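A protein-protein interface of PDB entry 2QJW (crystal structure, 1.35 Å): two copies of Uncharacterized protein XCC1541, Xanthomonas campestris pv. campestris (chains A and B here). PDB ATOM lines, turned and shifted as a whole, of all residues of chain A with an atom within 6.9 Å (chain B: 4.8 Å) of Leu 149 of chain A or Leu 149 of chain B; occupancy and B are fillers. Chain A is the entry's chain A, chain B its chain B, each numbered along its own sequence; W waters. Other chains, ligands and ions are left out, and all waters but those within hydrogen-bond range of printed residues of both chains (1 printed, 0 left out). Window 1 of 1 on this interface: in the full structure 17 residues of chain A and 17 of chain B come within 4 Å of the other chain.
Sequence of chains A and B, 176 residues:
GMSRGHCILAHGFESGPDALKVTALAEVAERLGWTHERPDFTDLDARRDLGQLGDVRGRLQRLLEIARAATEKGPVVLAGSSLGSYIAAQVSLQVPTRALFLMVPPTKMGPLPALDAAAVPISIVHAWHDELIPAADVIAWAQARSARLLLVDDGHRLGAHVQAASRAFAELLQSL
O of Ala 147 of chain B sits at hydrogen-bond distance from NE1 of Trp 128 of chain A. The backbone carbonyl oxygen (O) of Ala 147 of chain A is in hydrogen-bond range of the indole nitrogen (NE1) of Trp 128 of chain B. The backbone carbonyl oxygen of Leu 149 of chain A sits at hydrogen-bond distance from the backbone NH of Leu 151 of chain B. N of Leu 151 of chain A sits at hydrogen-bond distance from O of Leu 149 of chain B (2.8 Å).
The backbone carbonyl oxygen (O) of Arg 148 of chain A sits at hydrogen-bond distance from the backbone NH (N) of Ile 124 of chain A (2.9 Å). The backbone NH of Val 152 of chain A lies within hydrogen-bond range of the backbone carbonyl oxygen of His 126 of chain A. The backbone carbonyl oxygen (O) of Val 152 of chain A is in hydrogen-bond range of the backbone NH (N) of Trp 128 of chain A (2.9 Å). O of Ala 142 of chain A lies within hydrogen-bond range of N of Ala 147 of chain A, at 2.9 Å. N of Ile 124 of chain B is in hydrogen-bond range of O of Arg 148 of chain B (2.8 Å). The backbone NH of Leu 150 of chain B lies within hydrogen-bond range of the backbone carbonyl oxygen of Ile 124 of chain B (2.9 Å).
Among the printed residues, merely in contact across the chains: Leu 150 of chain A with Leu 149 of chain B (3.3 Å), Leu 151 of chain A with Arg 148 of chain B (3.4 Å), Leu 149 of chain A with Leu 150 of chain B (3.4 Å), Arg 148 of chain A with Leu 151 of chain B (3.4 Å), Gln 143 of chain A with Trp 128 of chain B (3.4 Å), Leu 149 of chain A with Leu 149 of chain B (3.5 Å), Arg 148 of chain A with Leu 150 of chain B (3.7 Å), Trp 128 of chain A with Ile 139 of chain B (3.7 Å), Leu 150 of chain A with Arg 148 of chain B (3.7 Å), Ile 139 of chain A with Trp 128 of chain B (3.8 Å), Ser 146 of chain A with Trp 128 of chain B (3.8 Å), Trp 128 of chain A with Ala 142 of chain B (3.8 Å), Ile 139 of chain A with Ile 139 of chain B (3.9 Å), Ala 142 of chain A with Trp 128 of chain B (3.9 Å) and Val 152 of chain A with Arg 148 of chain B (3.98 Å).
Of the printed residues of chain B, Ile 139 of chain A touches Trp 128 (3.8 Å) and Ile 139 (3.9 Å). Of the printed residues of chain B, Ala 142 of chain A touches Trp 128 (3.9 Å). Of chain B, only Leu 149 (3.5 Å), Leu 150 (3.4 Å) and Leu 151 (2.8 Å) come within 4 Å of Leu 149 of chain A. Printed residues of chain B within 4 Å of Leu 150 of chain A: Arg 148 (3.7 Å) and Leu 149 (3.3 Å). Leu 149 of chain B touches three residues of chain A. The nearest residue of chain B that does not touch Leu 149 of chain A is Trp 128 of chain B (4.2 Å). The nearest residue of chain A that does not touch Leu 149 of chain B is Trp 128 of chain A (4.2 Å).
Hydrophobic or aromatic side chains of chain B within 4 Å of the printed part of chain A: Trp 128, Ile 139, Ala 142, Leu 150 and Leu 151. Of the 21 printed residues of chain A, 11 touch a printed residue of chain B. Hydrophobic or aromatic side chains of chain A that line the printed part of chain B: Trp 128, Ile 139, Ala 142, Leu 150, Leu 151 and Val 152. Among the printed residues, no Asp or Glu carboxylate lies within 4 Å of a Lys or Arg side-chain nitrogen of the other chain.
Trp 128 of chain A touches Ile 139 of chain B, and with the chains exchanged Ile 139 of chain A touches Trp 128 of chain B. Trp 128 of chain A touches Ala 142 of chain B, and with the chains exchanged Ala 142 of chain A touches Trp 128 of chain B. Arg 148 of chain A touches Leu 150 of chain B, and with the chains exchanged Leu 150 of chain A touches Arg 148 of chain B. Arg 148 of chain A touches Leu 151 of chain B, and with the chains exchanged Leu 151 of chain A touches Arg 148 of chain B. Positions printed for both chains: 124, 126, 128, 138, 139, 142, 147, 148, 149, 150 and 151. Of the 19 pairs that touch across the chains among the printed residues, 16 have their exchanged pair printed and touching as well.
Water W1 bridges O of Trp 128 of chain B and NE2 of Gln 143 of chain A.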
ATOM      1  N   LEU A 102     -11.337 -24.442 -20.119  1.00  0.00           N
ATOM      2  CA  LEU A 102     -11.204 -22.981 -20.173  1.00  0.00           C
ATOM      3  C   LEU A 102     -10.210 -22.477 -19.186  1.00  0.00           C
ATOM      4  O   LEU A 102     -10.364 -22.634 -17.999  1.00  0.00           O
ATOM      5  CB  LEU A 102     -12.534 -22.357 -19.849  1.00  0.00           C
ATOM      6  CG  LEU A 102     -13.793 -22.829 -20.574  1.00  0.00           C
ATOM      7  CD1 LEU A 102     -15.106 -22.119 -20.130  1.00  0.00           C
ATOM      8  CD2 LEU A 102     -13.612 -22.636 -22.085  1.00  0.00           C
ATOM      9  N   PRO A 105     -11.209 -17.692 -18.312  1.00  0.00           N
ATOM     10  CA  PRO A 105     -12.276 -17.246 -19.213  1.00  0.00           C
ATOM     11  C   PRO A 105     -12.881 -15.906 -18.801  1.00  0.00           C
ATOM     12  O   PRO A 105     -13.230 -15.762 -17.655  1.00  0.00           O
ATOM     13  CB  PRO A 105     -13.319 -18.377 -19.075  1.00  0.00           C
ATOM     14  CG  PRO A 105     -13.183 -18.865 -17.744  1.00  0.00           C
ATOM     15  CD  PRO A 105     -11.686 -18.789 -17.444  1.00  0.00           C
ATOM     16  N   ILE A 122     -17.321 -29.211 -18.331  1.00  0.00           N
ATOM     17  CA  ILE A 122     -16.516 -27.978 -18.362  1.00  0.00           C
ATOM     18  C   ILE A 122     -15.526 -28.039 -17.224  1.00  0.00           C
ATOM     19  O   ILE A 122     -15.925 -28.342 -16.087  1.00  0.00           O
ATOM     20  CB  ILE A 122     -17.376 -26.722 -18.227  1.00  0.00           C
ATOM     21  CG1 ILE A 122     -18.428 -26.676 -19.372  1.00  0.00           C
ATOM     22  CG2 ILE A 122     -16.526 -25.461 -18.174  1.00  0.00           C
ATOM     23  CD1 ILE A 122     -19.524 -25.624 -19.151  1.00  0.00           C
ATOM     24  N   SER A 123     -14.257 -27.785 -17.540  1.00  0.00           N
ATOM     25  CA  SER A 123     -13.193 -27.687 -16.552  1.00  0.00           C
ATOM     26  C   SER A 123     -12.507 -26.349 -16.760  1.00  0.00           C
ATOM     27  O   SER A 123     -12.148 -26.033 -17.876  1.00  0.00           O
ATOM     28  CB  SER A 123     -12.240 -28.841 -16.668  1.00  0.00           C
ATOM     29  OG  SER A 123     -11.180 -28.752 -15.764  1.00  0.00           O
ATOM     30  N   ILE A 124     -12.326 -25.599 -15.671  1.00  0.00           N
ATOM     31  CA  ILE A 124     -11.822 -24.240 -15.704  1.00  0.00           C
ATOM     32  C   ILE A 124     -10.608 -24.168 -14.808  1.00  0.00           C
ATOM     33  O   ILE A 124     -10.608 -24.724 -13.703  1.00  0.00           O
ATOM     34  CB  ILE A 124     -12.904 -23.217 -15.212  1.00  0.00           C
ATOM     35  CG1 ILE A 124     -14.216 -23.347 -15.997  1.00  0.00           C
ATOM     36  CG2 ILE A 124     -12.358 -21.779 -15.231  1.00  0.00           C
ATOM     37  CD1 ILE A 124     -15.371 -22.680 -15.264  1.00  0.00           C
ATOM     38  N   VAL A 125      -9.597 -23.458 -15.274  1.00  0.00           N
ATOM     39  CA  VAL A 125      -8.437 -23.048 -14.447  1.00  0.00           C
ATOM     40  C   VAL A 125      -8.455 -21.528 -14.403  1.00  0.00           C
ATOM     41  O   VAL A 125      -8.358 -20.912 -15.439  1.00  0.00           O
ATOM     42  CB  VAL A 125      -7.070 -23.570 -14.908  1.00  0.00           C
ATOM     43  CG1 VAL A 125      -5.944 -23.105 -13.978  1.00  0.00           C
ATOM     44  CG2 VAL A 125      -7.144 -25.089 -14.962  1.00  0.00           C
ATOM     45  N   HIS A 126      -8.612 -20.950 -13.189  1.00  0.00           N
ATOM     46  CA  HIS A 126      -8.553 -19.494 -13.057  1.00  0.00           C
ATOM     47  C   HIS A 126      -7.602 -19.082 -11.981  1.00  0.00           C
ATOM     48  O   HIS A 126      -7.220 -19.830 -11.096  1.00  0.00           O
ATOM     49  CB  HIS A 126      -9.933 -18.962 -12.758  1.00  0.00           C
ATOM     50  CG  HIS A 126     -10.083 -17.525 -13.054  1.00  0.00           C
ATOM     51  ND1 HIS A 126     -10.008 -17.049 -14.333  1.00  0.00           N
ATOM     52  CD2 HIS A 126     -10.313 -16.464 -12.246  1.00  0.00           C
ATOM     53  CE1 HIS A 126     -10.150 -15.727 -14.292  1.00  0.00           C
ATOM     54  NE2 HIS A 126     -10.318 -15.361 -13.035  1.00  0.00           N
ATOM     55  N   TRP A 128      -6.510 -16.743  -8.845  1.00  0.00           N
ATOM     56  CA  TRP A 128      -7.030 -15.989  -7.741  1.00  0.00           C
ATOM     57  C   TRP A 128      -6.789 -14.486  -7.944  1.00  0.00           C
ATOM     58  O   TRP A 128      -7.675 -13.705  -7.512  1.00  0.00           O
ATOM     59  CB  TRP A 128      -6.317 -16.382  -6.440  1.00  0.00           C
ATOM     60  CG  TRP A 128      -6.820 -17.586  -5.746  1.00  0.00           C
ATOM     61  CD1 TRP A 128      -6.105 -18.672  -5.411  1.00  0.00           C
ATOM     62  CD2 TRP A 128      -8.144 -17.815  -5.258  1.00  0.00           C
ATOM     63  NE1 TRP A 128      -6.893 -19.590  -4.767  1.00  0.00           N
ATOM     64  CE2 TRP A 128      -8.145 -19.077  -4.628  1.00  0.00           C
ATOM     65  CE3 TRP A 128      -9.333 -17.054  -5.238  1.00  0.00           C
ATOM     66  CZ2 TRP A 128      -9.242 -19.591  -4.045  1.00  0.00           C
ATOM     67  CZ3 TRP A 128     -10.441 -17.594  -4.617  1.00  0.00           C
ATOM     68  CH2 TRP A 128     -10.384 -18.845  -4.037  1.00  0.00           C
ATOM     69  N   ALA A 135     -11.826 -13.039  -9.924  1.00  0.00           N
ATOM     70  CA  ALA A 135     -12.085 -14.453  -9.616  1.00  0.00           C
ATOM     71  C   ALA A 135     -13.552 -14.678  -9.263  1.00  0.00           C
ATOM     72  O   ALA A 135     -14.152 -15.704  -9.611  1.00  0.00           O
ATOM     73  CB  ALA A 135     -11.207 -14.924  -8.466  1.00  0.00           C
ATOM     74  N   VAL A 138     -15.785 -15.521 -12.257  1.00  0.00           N
ATOM     75  CA  VAL A 138     -15.645 -16.912 -12.767  1.00  0.00           C
ATOM     76  C   VAL A 138     -16.183 -17.922 -11.782  1.00  0.00           C
ATOM     77  O   VAL A 138     -16.886 -18.877 -12.155  1.00  0.00           O
ATOM     78  CB  VAL A 138     -14.181 -17.171 -13.096  1.00  0.00           C
ATOM     79  CG1 VAL A 138     -13.934 -18.663 -13.486  1.00  0.00           C
ATOM     80  CG2 VAL A 138     -13.726 -16.268 -14.235  1.00  0.00           C
ATOM     81  N   ILE A 139     -15.993 -17.699 -10.486  1.00  0.00           N
ATOM     82  CA  ILE A 139     -16.576 -18.520  -9.467  1.00  0.00           C
ATOM     83  C   ILE A 139     -18.105 -18.520  -9.642  1.00  0.00           C
ATOM     84  O   ILE A 139     -18.753 -19.582  -9.656  1.00  0.00           O
ATOM     85  CB  ILE A 139     -16.200 -18.031  -8.036  1.00  0.00           C
ATOM     86  CG1 ILE A 139     -14.699 -18.352  -7.827  1.00  0.00           C
ATOM     87  CG2 ILE A 139     -17.157 -18.652  -6.992  1.00  0.00           C
ATOM     88  CD1 ILE A 139     -14.024 -17.480  -6.718  1.00  0.00           C
ATOM     89  N   ALA A 140     -18.741 -17.346  -9.847  1.00  0.00           N
ATOM     90  CA  ALA A 140     -20.213 -17.312  -9.997  1.00  0.00           C
ATOM     91  C   ALA A 140     -20.675 -18.051 -11.269  1.00  0.00           C
ATOM     92  O   ALA A 140     -21.678 -18.746 -11.272  1.00  0.00           O
ATOM     93  CB  ALA A 140     -20.759 -15.881  -9.951  1.00  0.00           C
ATOM     94  N   ALA A 142     -19.081 -20.458 -12.901  1.00  0.00           N
ATOM     95  CA  ALA A 142     -18.896 -21.871 -12.705  1.00  0.00           C
ATOM     96  C   ALA A 142     -19.901 -22.484 -11.730  1.00  0.00           C
ATOM     97  O   ALA A 142     -20.414 -23.598 -11.928  1.00  0.00           O
ATOM     98  CB  ALA A 142     -17.457 -22.144 -12.215  1.00  0.00           C
ATOM     99  N   GLN A 143     -20.178 -21.778 -10.637  1.00  0.00           N
ATOM    100  CA  GLN A 143     -21.126 -22.264  -9.604  1.00  0.00           C
ATOM    101  C   GLN A 143     -22.527 -22.517 -10.210  1.00  0.00           C
ATOM    102  O   GLN A 143     -23.202 -23.508  -9.885  1.00  0.00           O
ATOM    103  CB  GLN A 143     -21.191 -21.305  -8.428  1.00  0.00           C
ATOM    104  CG  GLN A 143     -22.043 -21.812  -7.261  1.00  0.00           C
ATOM    105  CD  GLN A 143     -21.658 -21.191  -5.935  1.00  0.00           C
ATOM    106  OE1 GLN A 143     -21.105 -20.105  -5.875  1.00  0.00           O
ATOM    107  NE2 GLN A 143     -21.944 -21.904  -4.855  1.00  0.00           N
ATOM    108  N   SER A 146     -22.232 -25.757 -11.995  1.00  0.00           N
ATOM    109  CA  SER A 146     -21.442 -26.742 -11.273  1.00  0.00           C
ATOM    110  C   SER A 146     -20.237 -27.191 -12.123  1.00  0.00           C
ATOM    111  O   SER A 146     -19.858 -28.328 -12.071  1.00  0.00           O
ATOM    112  CB  SER A 146     -22.292 -27.935 -10.841  1.00  0.00           C
ATOM    113  OG  SER A 146     -23.393 -27.491 -10.031  1.00  0.00           O
ATOM    114  N   ALA A 147     -19.542 -26.266 -12.827  1.00  0.00           N
ATOM    115  CA  ALA A 147     -18.383 -26.614 -13.631  1.00  0.00           C
ATOM    116  C   ALA A 147     -17.220 -26.857 -12.722  1.00  0.00           C
ATOM    117  O   ALA A 147     -17.131 -26.265 -11.640  1.00  0.00           O
ATOM    118  CB  ALA A 147     -17.992 -25.475 -14.560  1.00  0.00           C
ATOM    119  N   ARG A 148     -16.355 -27.812 -13.054  1.00  0.00           N
ATOM    120  CA  ARG A 148     -15.146 -28.046 -12.273  1.00  0.00           C
ATOM    121  C   ARG A 148     -14.327 -26.759 -12.372  1.00  0.00           C
ATOM    122  O   ARG A 148     -14.128 -26.228 -13.451  1.00  0.00           O
ATOM    123  CB  ARG A 148     -14.345 -29.270 -12.690  1.00  0.00           C
ATOM    124  CG  ARG A 148     -13.185 -29.615 -11.761  1.00  0.00           C
ATOM    125  CD  ARG A 148     -12.552 -30.923 -12.084  1.00  0.00           C
ATOM    126  NE  ARG A 148     -13.534 -31.980 -11.906  1.00  0.00           N
ATOM    127  CZ  ARG A 148     -13.290 -33.281 -12.012  1.00  0.00           C
ATOM    128  NH1 ARG A 148     -12.078 -33.738 -12.276  1.00  0.00           N
ATOM    129  NH2 ARG A 148     -14.307 -34.130 -11.920  1.00  0.00           N
ATOM    130  N   LEU A 149     -13.823 -26.333 -11.218  1.00  0.00           N
ATOM    131  CA  LEU A 149     -13.058 -25.075 -11.118  1.00  0.00           C
ATOM    132  C   LEU A 149     -11.850 -25.270 -10.258  1.00  0.00           C
ATOM    133  O   LEU A 149     -11.960 -25.661  -9.117  1.00  0.00           O
ATOM    134  CB  LEU A 149     -13.903 -23.959 -10.547  1.00  0.00           C
ATOM    135  CG  LEU A 149     -13.235 -22.585 -10.360  1.00  0.00           C
ATOM    136  CD1 LEU A 149     -12.640 -22.028 -11.615  1.00  0.00           C
ATOM    137  CD2 LEU A 149     -14.307 -21.606  -9.813  1.00  0.00           C
ATOM    138  N   LEU A 150     -10.698 -24.951 -10.834  1.00  0.00           N
ATOM    139  CA  LEU A 150      -9.387 -24.924 -10.134  1.00  0.00           C
ATOM    140  C   LEU A 150      -8.876 -23.508 -10.071  1.00  0.00           C
ATOM    141  O   LEU A 150      -8.762 -22.868 -11.108  1.00  0.00           O
ATOM    142  CB  LEU A 150      -8.331 -25.782 -10.843  1.00  0.00           C
ATOM    143  CG  LEU A 150      -6.951 -25.829 -10.230  1.00  0.00           C
ATOM    144  CD1 LEU A 150      -7.056 -26.609  -8.930  1.00  0.00           C
ATOM    145  CD2 LEU A 150      -5.945 -26.496 -11.171  1.00  0.00           C
ATOM    146  N   LEU A 151      -8.714 -23.041  -8.845  1.00  0.00           N
ATOM    147  CA  LEU A 151      -8.195 -21.699  -8.545  1.00  0.00           C
ATOM    148  C   LEU A 151      -6.783 -21.879  -8.051  1.00  0.00           C
ATOM    149  O   LEU A 151      -6.531 -22.583  -7.079  1.00  0.00           O
ATOM    150  CB  LEU A 151      -9.115 -20.985  -7.524  1.00  0.00           C
ATOM    151  CG  LEU A 151     -10.498 -20.631  -8.067  1.00  0.00           C
ATOM    152  CD1 LEU A 151     -11.546 -20.756  -7.010  1.00  0.00           C
ATOM    153  CD2 LEU A 151     -10.429 -19.236  -8.696  1.00  0.00           C
ATOM    154  N   VAL A 152      -5.908 -21.107  -8.670  1.00  0.00           N
ATOM    155  CA  VAL A 152      -4.475 -21.139  -8.360  1.00  0.00           C
ATOM    156  C   VAL A 152      -3.927 -19.762  -7.993  1.00  0.00           C
ATOM    157  O   VAL A 152      -4.492 -18.728  -8.365  1.00  0.00           O
ATOM    158  CB  VAL A 152      -3.631 -21.712  -9.527  1.00  0.00           C
ATOM    159  CG1 VAL A 152      -4.044 -23.149  -9.870  1.00  0.00           C
ATOM    160  CG2 VAL A 152      -3.764 -20.871 -10.787  1.00  0.00           C
ATOM    161  N   ILE B 124      -6.810 -27.802  -1.512  1.00  0.00           N
ATOM    162  CA  ILE B 124      -8.168 -28.087  -1.026  1.00  0.00           C
ATOM    163  C   ILE B 124      -9.034 -28.610  -2.133  1.00  0.00           C
ATOM    164  O   ILE B 124      -8.950 -28.149  -3.248  1.00  0.00           O
ATOM    165  CB  ILE B 124      -8.862 -26.795  -0.514  1.00  0.00           C
ATOM    166  CG1 ILE B 124      -7.969 -26.101   0.526  1.00  0.00           C
ATOM    167  CG2 ILE B 124     -10.228 -27.058   0.052  1.00  0.00           C
ATOM    168  CD1 ILE B 124      -8.496 -24.661   0.892  1.00  0.00           C
ATOM    169  N   HIS B 126     -13.086 -29.195  -2.560  1.00  0.00           N
ATOM    170  CA  HIS B 126     -14.385 -28.916  -1.955  1.00  0.00           C
ATOM    171  C   HIS B 126     -15.488 -29.210  -2.952  1.00  0.00           C
ATOM    172  O   HIS B 126     -15.220 -29.330  -4.144  1.00  0.00           O
ATOM    173  CB  HIS B 126     -14.477 -27.491  -1.403  1.00  0.00           C
ATOM    174  CG  HIS B 126     -15.557 -27.361  -0.387  1.00  0.00           C
ATOM    175  ND1 HIS B 126     -15.487 -28.013   0.826  1.00  0.00           N
ATOM    176  CD2 HIS B 126     -16.729 -26.682  -0.397  1.00  0.00           C
ATOM    177  CE1 HIS B 126     -16.601 -27.755   1.503  1.00  0.00           C
ATOM    178  NE2 HIS B 126     -17.355 -26.939   0.797  1.00  0.00           N
ATOM    179  N   TRP B 128     -19.218 -28.366  -4.650  1.00  0.00           N
ATOM    180  CA  TRP B 128     -20.142 -27.278  -4.854  1.00  0.00           C
ATOM    181  C   TRP B 128     -21.419 -27.386  -4.037  1.00  0.00           C
ATOM    182  O   TRP B 128     -21.988 -26.349  -3.651  1.00  0.00           O
ATOM    183  CB  TRP B 128     -20.542 -27.177  -6.320  1.00  0.00           C
ATOM    184  CG  TRP B 128     -19.568 -26.555  -7.273  1.00  0.00           C
ATOM    185  CD1 TRP B 128     -19.035 -27.154  -8.350  1.00  0.00           C
ATOM    186  CD2 TRP B 128     -19.097 -25.208  -7.290  1.00  0.00           C
ATOM    187  NE1 TRP B 128     -18.231 -26.297  -9.028  1.00  0.00           N
ATOM    188  CE2 TRP B 128     -18.279 -25.074  -8.415  1.00  0.00           C
ATOM    189  CE3 TRP B 128     -19.296 -24.077  -6.459  1.00  0.00           C
ATOM    190  CZ2 TRP B 128     -17.658 -23.891  -8.726  1.00  0.00           C
ATOM    191  CZ3 TRP B 128     -18.655 -22.908  -6.741  1.00  0.00           C
ATOM    192  CH2 TRP B 128     -17.857 -22.803  -7.894  1.00  0.00           C
ATOM    193  N   VAL B 138     -15.647 -21.937   2.103  1.00  0.00           N
ATOM    194  CA  VAL B 138     -14.353 -22.460   1.801  1.00  0.00           C
ATOM    195  C   VAL B 138     -13.642 -21.572   0.791  1.00  0.00           C
ATOM    196  O   VAL B 138     -12.431 -21.345   0.870  1.00  0.00           O
ATOM    197  CB  VAL B 138     -14.471 -23.885   1.317  1.00  0.00           C
ATOM    198  CG1 VAL B 138     -13.118 -24.435   0.808  1.00  0.00           C
ATOM    199  CG2 VAL B 138     -14.964 -24.809   2.472  1.00  0.00           C
ATOM    200  N   ILE B 139     -14.384 -21.074  -0.193  1.00  0.00           N
ATOM    201  CA  ILE B 139     -13.788 -20.120  -1.171  1.00  0.00           C
ATOM    202  C   ILE B 139     -13.212 -18.901  -0.496  1.00  0.00           C
ATOM    203  O   ILE B 139     -12.122 -18.524  -0.783  1.00  0.00           O
ATOM    204  CB  ILE B 139     -14.863 -19.720  -2.231  1.00  0.00           C
ATOM    205  CG1 ILE B 139     -15.172 -20.951  -3.125  1.00  0.00           C
ATOM    206  CG2 ILE B 139     -14.432 -18.477  -3.000  1.00  0.00           C
ATOM    207  CD1 ILE B 139     -16.545 -20.813  -3.827  1.00  0.00           C
ATOM    208  N   ALA B 142      -9.960 -20.005   1.384  1.00  0.00           N
ATOM    209  CA  ALA B 142      -8.889 -20.259   0.476  1.00  0.00           C
ATOM    210  C   ALA B 142      -8.394 -18.961  -0.161  1.00  0.00           C
ATOM    211  O   ALA B 142      -7.182 -18.765  -0.326  1.00  0.00           O
ATOM    212  CB  ALA B 142      -9.349 -21.250  -0.604  1.00  0.00           C
ATOM    213  N   ALA B 147      -4.880 -20.275  -1.238  1.00  0.00           N
ATOM    214  CA  ALA B 147      -4.737 -21.738  -1.245  1.00  0.00           C
ATOM    215  C   ALA B 147      -5.243 -22.317  -2.549  1.00  0.00           C
ATOM    216  O   ALA B 147      -6.230 -21.826  -3.089  1.00  0.00           O
ATOM    217  CB  ALA B 147      -5.478 -22.367  -0.124  1.00  0.00           C
ATOM    218  N   ARG B 148      -4.563 -23.313  -3.109  1.00  0.00           N
ATOM    219  CA  ARG B 148      -5.097 -23.952  -4.332  1.00  0.00           C
ATOM    220  C   ARG B 148      -6.401 -24.669  -3.963  1.00  0.00           C
ATOM    221  O   ARG B 148      -6.426 -25.425  -2.989  1.00  0.00           O
ATOM    222  CB  ARG B 148      -4.150 -24.937  -4.954  1.00  0.00           C
ATOM    223  CG  ARG B 148      -4.616 -25.453  -6.340  1.00  0.00           C
ATOM    224  CD  ARG B 148      -3.571 -26.368  -6.951  1.00  0.00           C
ATOM    225  NE  ARG B 148      -2.343 -25.638  -7.277  1.00  0.00           N
ATOM    226  CZ  ARG B 148      -1.292 -26.138  -7.946  1.00  0.00           C
ATOM    227  NH1 ARG B 148      -1.281 -27.380  -8.408  1.00  0.00           N
ATOM    228  NH2 ARG B 148      -0.233 -25.369  -8.124  1.00  0.00           N
ATOM    229  N   LEU B 149      -7.451 -24.404  -4.742  1.00  0.00           N
ATOM    230  CA  LEU B 149      -8.797 -24.897  -4.481  1.00  0.00           C
ATOM    231  C   LEU B 149      -9.389 -25.482  -5.737  1.00  0.00           C
ATOM    232  O   LEU B 149      -9.438 -24.814  -6.792  1.00  0.00           O
ATOM    233  CB  LEU B 149      -9.687 -23.752  -4.003  1.00  0.00           C
ATOM    234  CG  LEU B 149     -11.162 -24.021  -3.779  1.00  0.00           C
ATOM    235  CD1 LEU B 149     -11.331 -25.121  -2.741  1.00  0.00           C
ATOM    236  CD2 LEU B 149     -11.917 -22.756  -3.334  1.00  0.00           C
ATOM    237  N   LEU B 150      -9.835 -26.734  -5.590  1.00  0.00           N
ATOM    238  CA  LEU B 150     -10.583 -27.488  -6.618  1.00  0.00           C
ATOM    239  C   LEU B 150     -11.996 -27.641  -6.131  1.00  0.00           C
ATOM    240  O   LEU B 150     -12.212 -28.175  -5.017  1.00  0.00           O
ATOM    241  CB  LEU B 150      -9.946 -28.831  -6.905  1.00  0.00           C
ATOM    242  CG  LEU B 150     -10.646 -29.698  -7.937  1.00  0.00           C
ATOM    243  CD1 LEU B 150     -10.520 -29.040  -9.294  1.00  0.00           C
ATOM    244  CD2 LEU B 150     -10.012 -31.094  -7.970  1.00  0.00           C
ATOM    245  N   LEU B 151     -12.935 -27.164  -6.936  1.00  0.00           N
ATOM    246  CA  LEU B 151     -14.374 -27.275  -6.672  1.00  0.00           C
ATOM    247  C   LEU B 151     -14.965 -28.256  -7.648  1.00  0.00           C
ATOM    248  O   LEU B 151     -14.816 -28.075  -8.871  1.00  0.00           O
ATOM    249  CB  LEU B 151     -15.066 -25.929  -6.783  1.00  0.00           C
ATOM    250  CG  LEU B 151     -14.728 -24.988  -5.625  1.00  0.00           C
ATOM    251  CD1 LEU B 151     -14.623 -23.550  -6.100  1.00  0.00           C
ATOM    252  CD2 LEU B 151     -15.687 -25.141  -4.486  1.00  0.00           C
HETATM  253  O   HOH W   1     -23.065 -24.470  -5.271  1.00  0.00           O
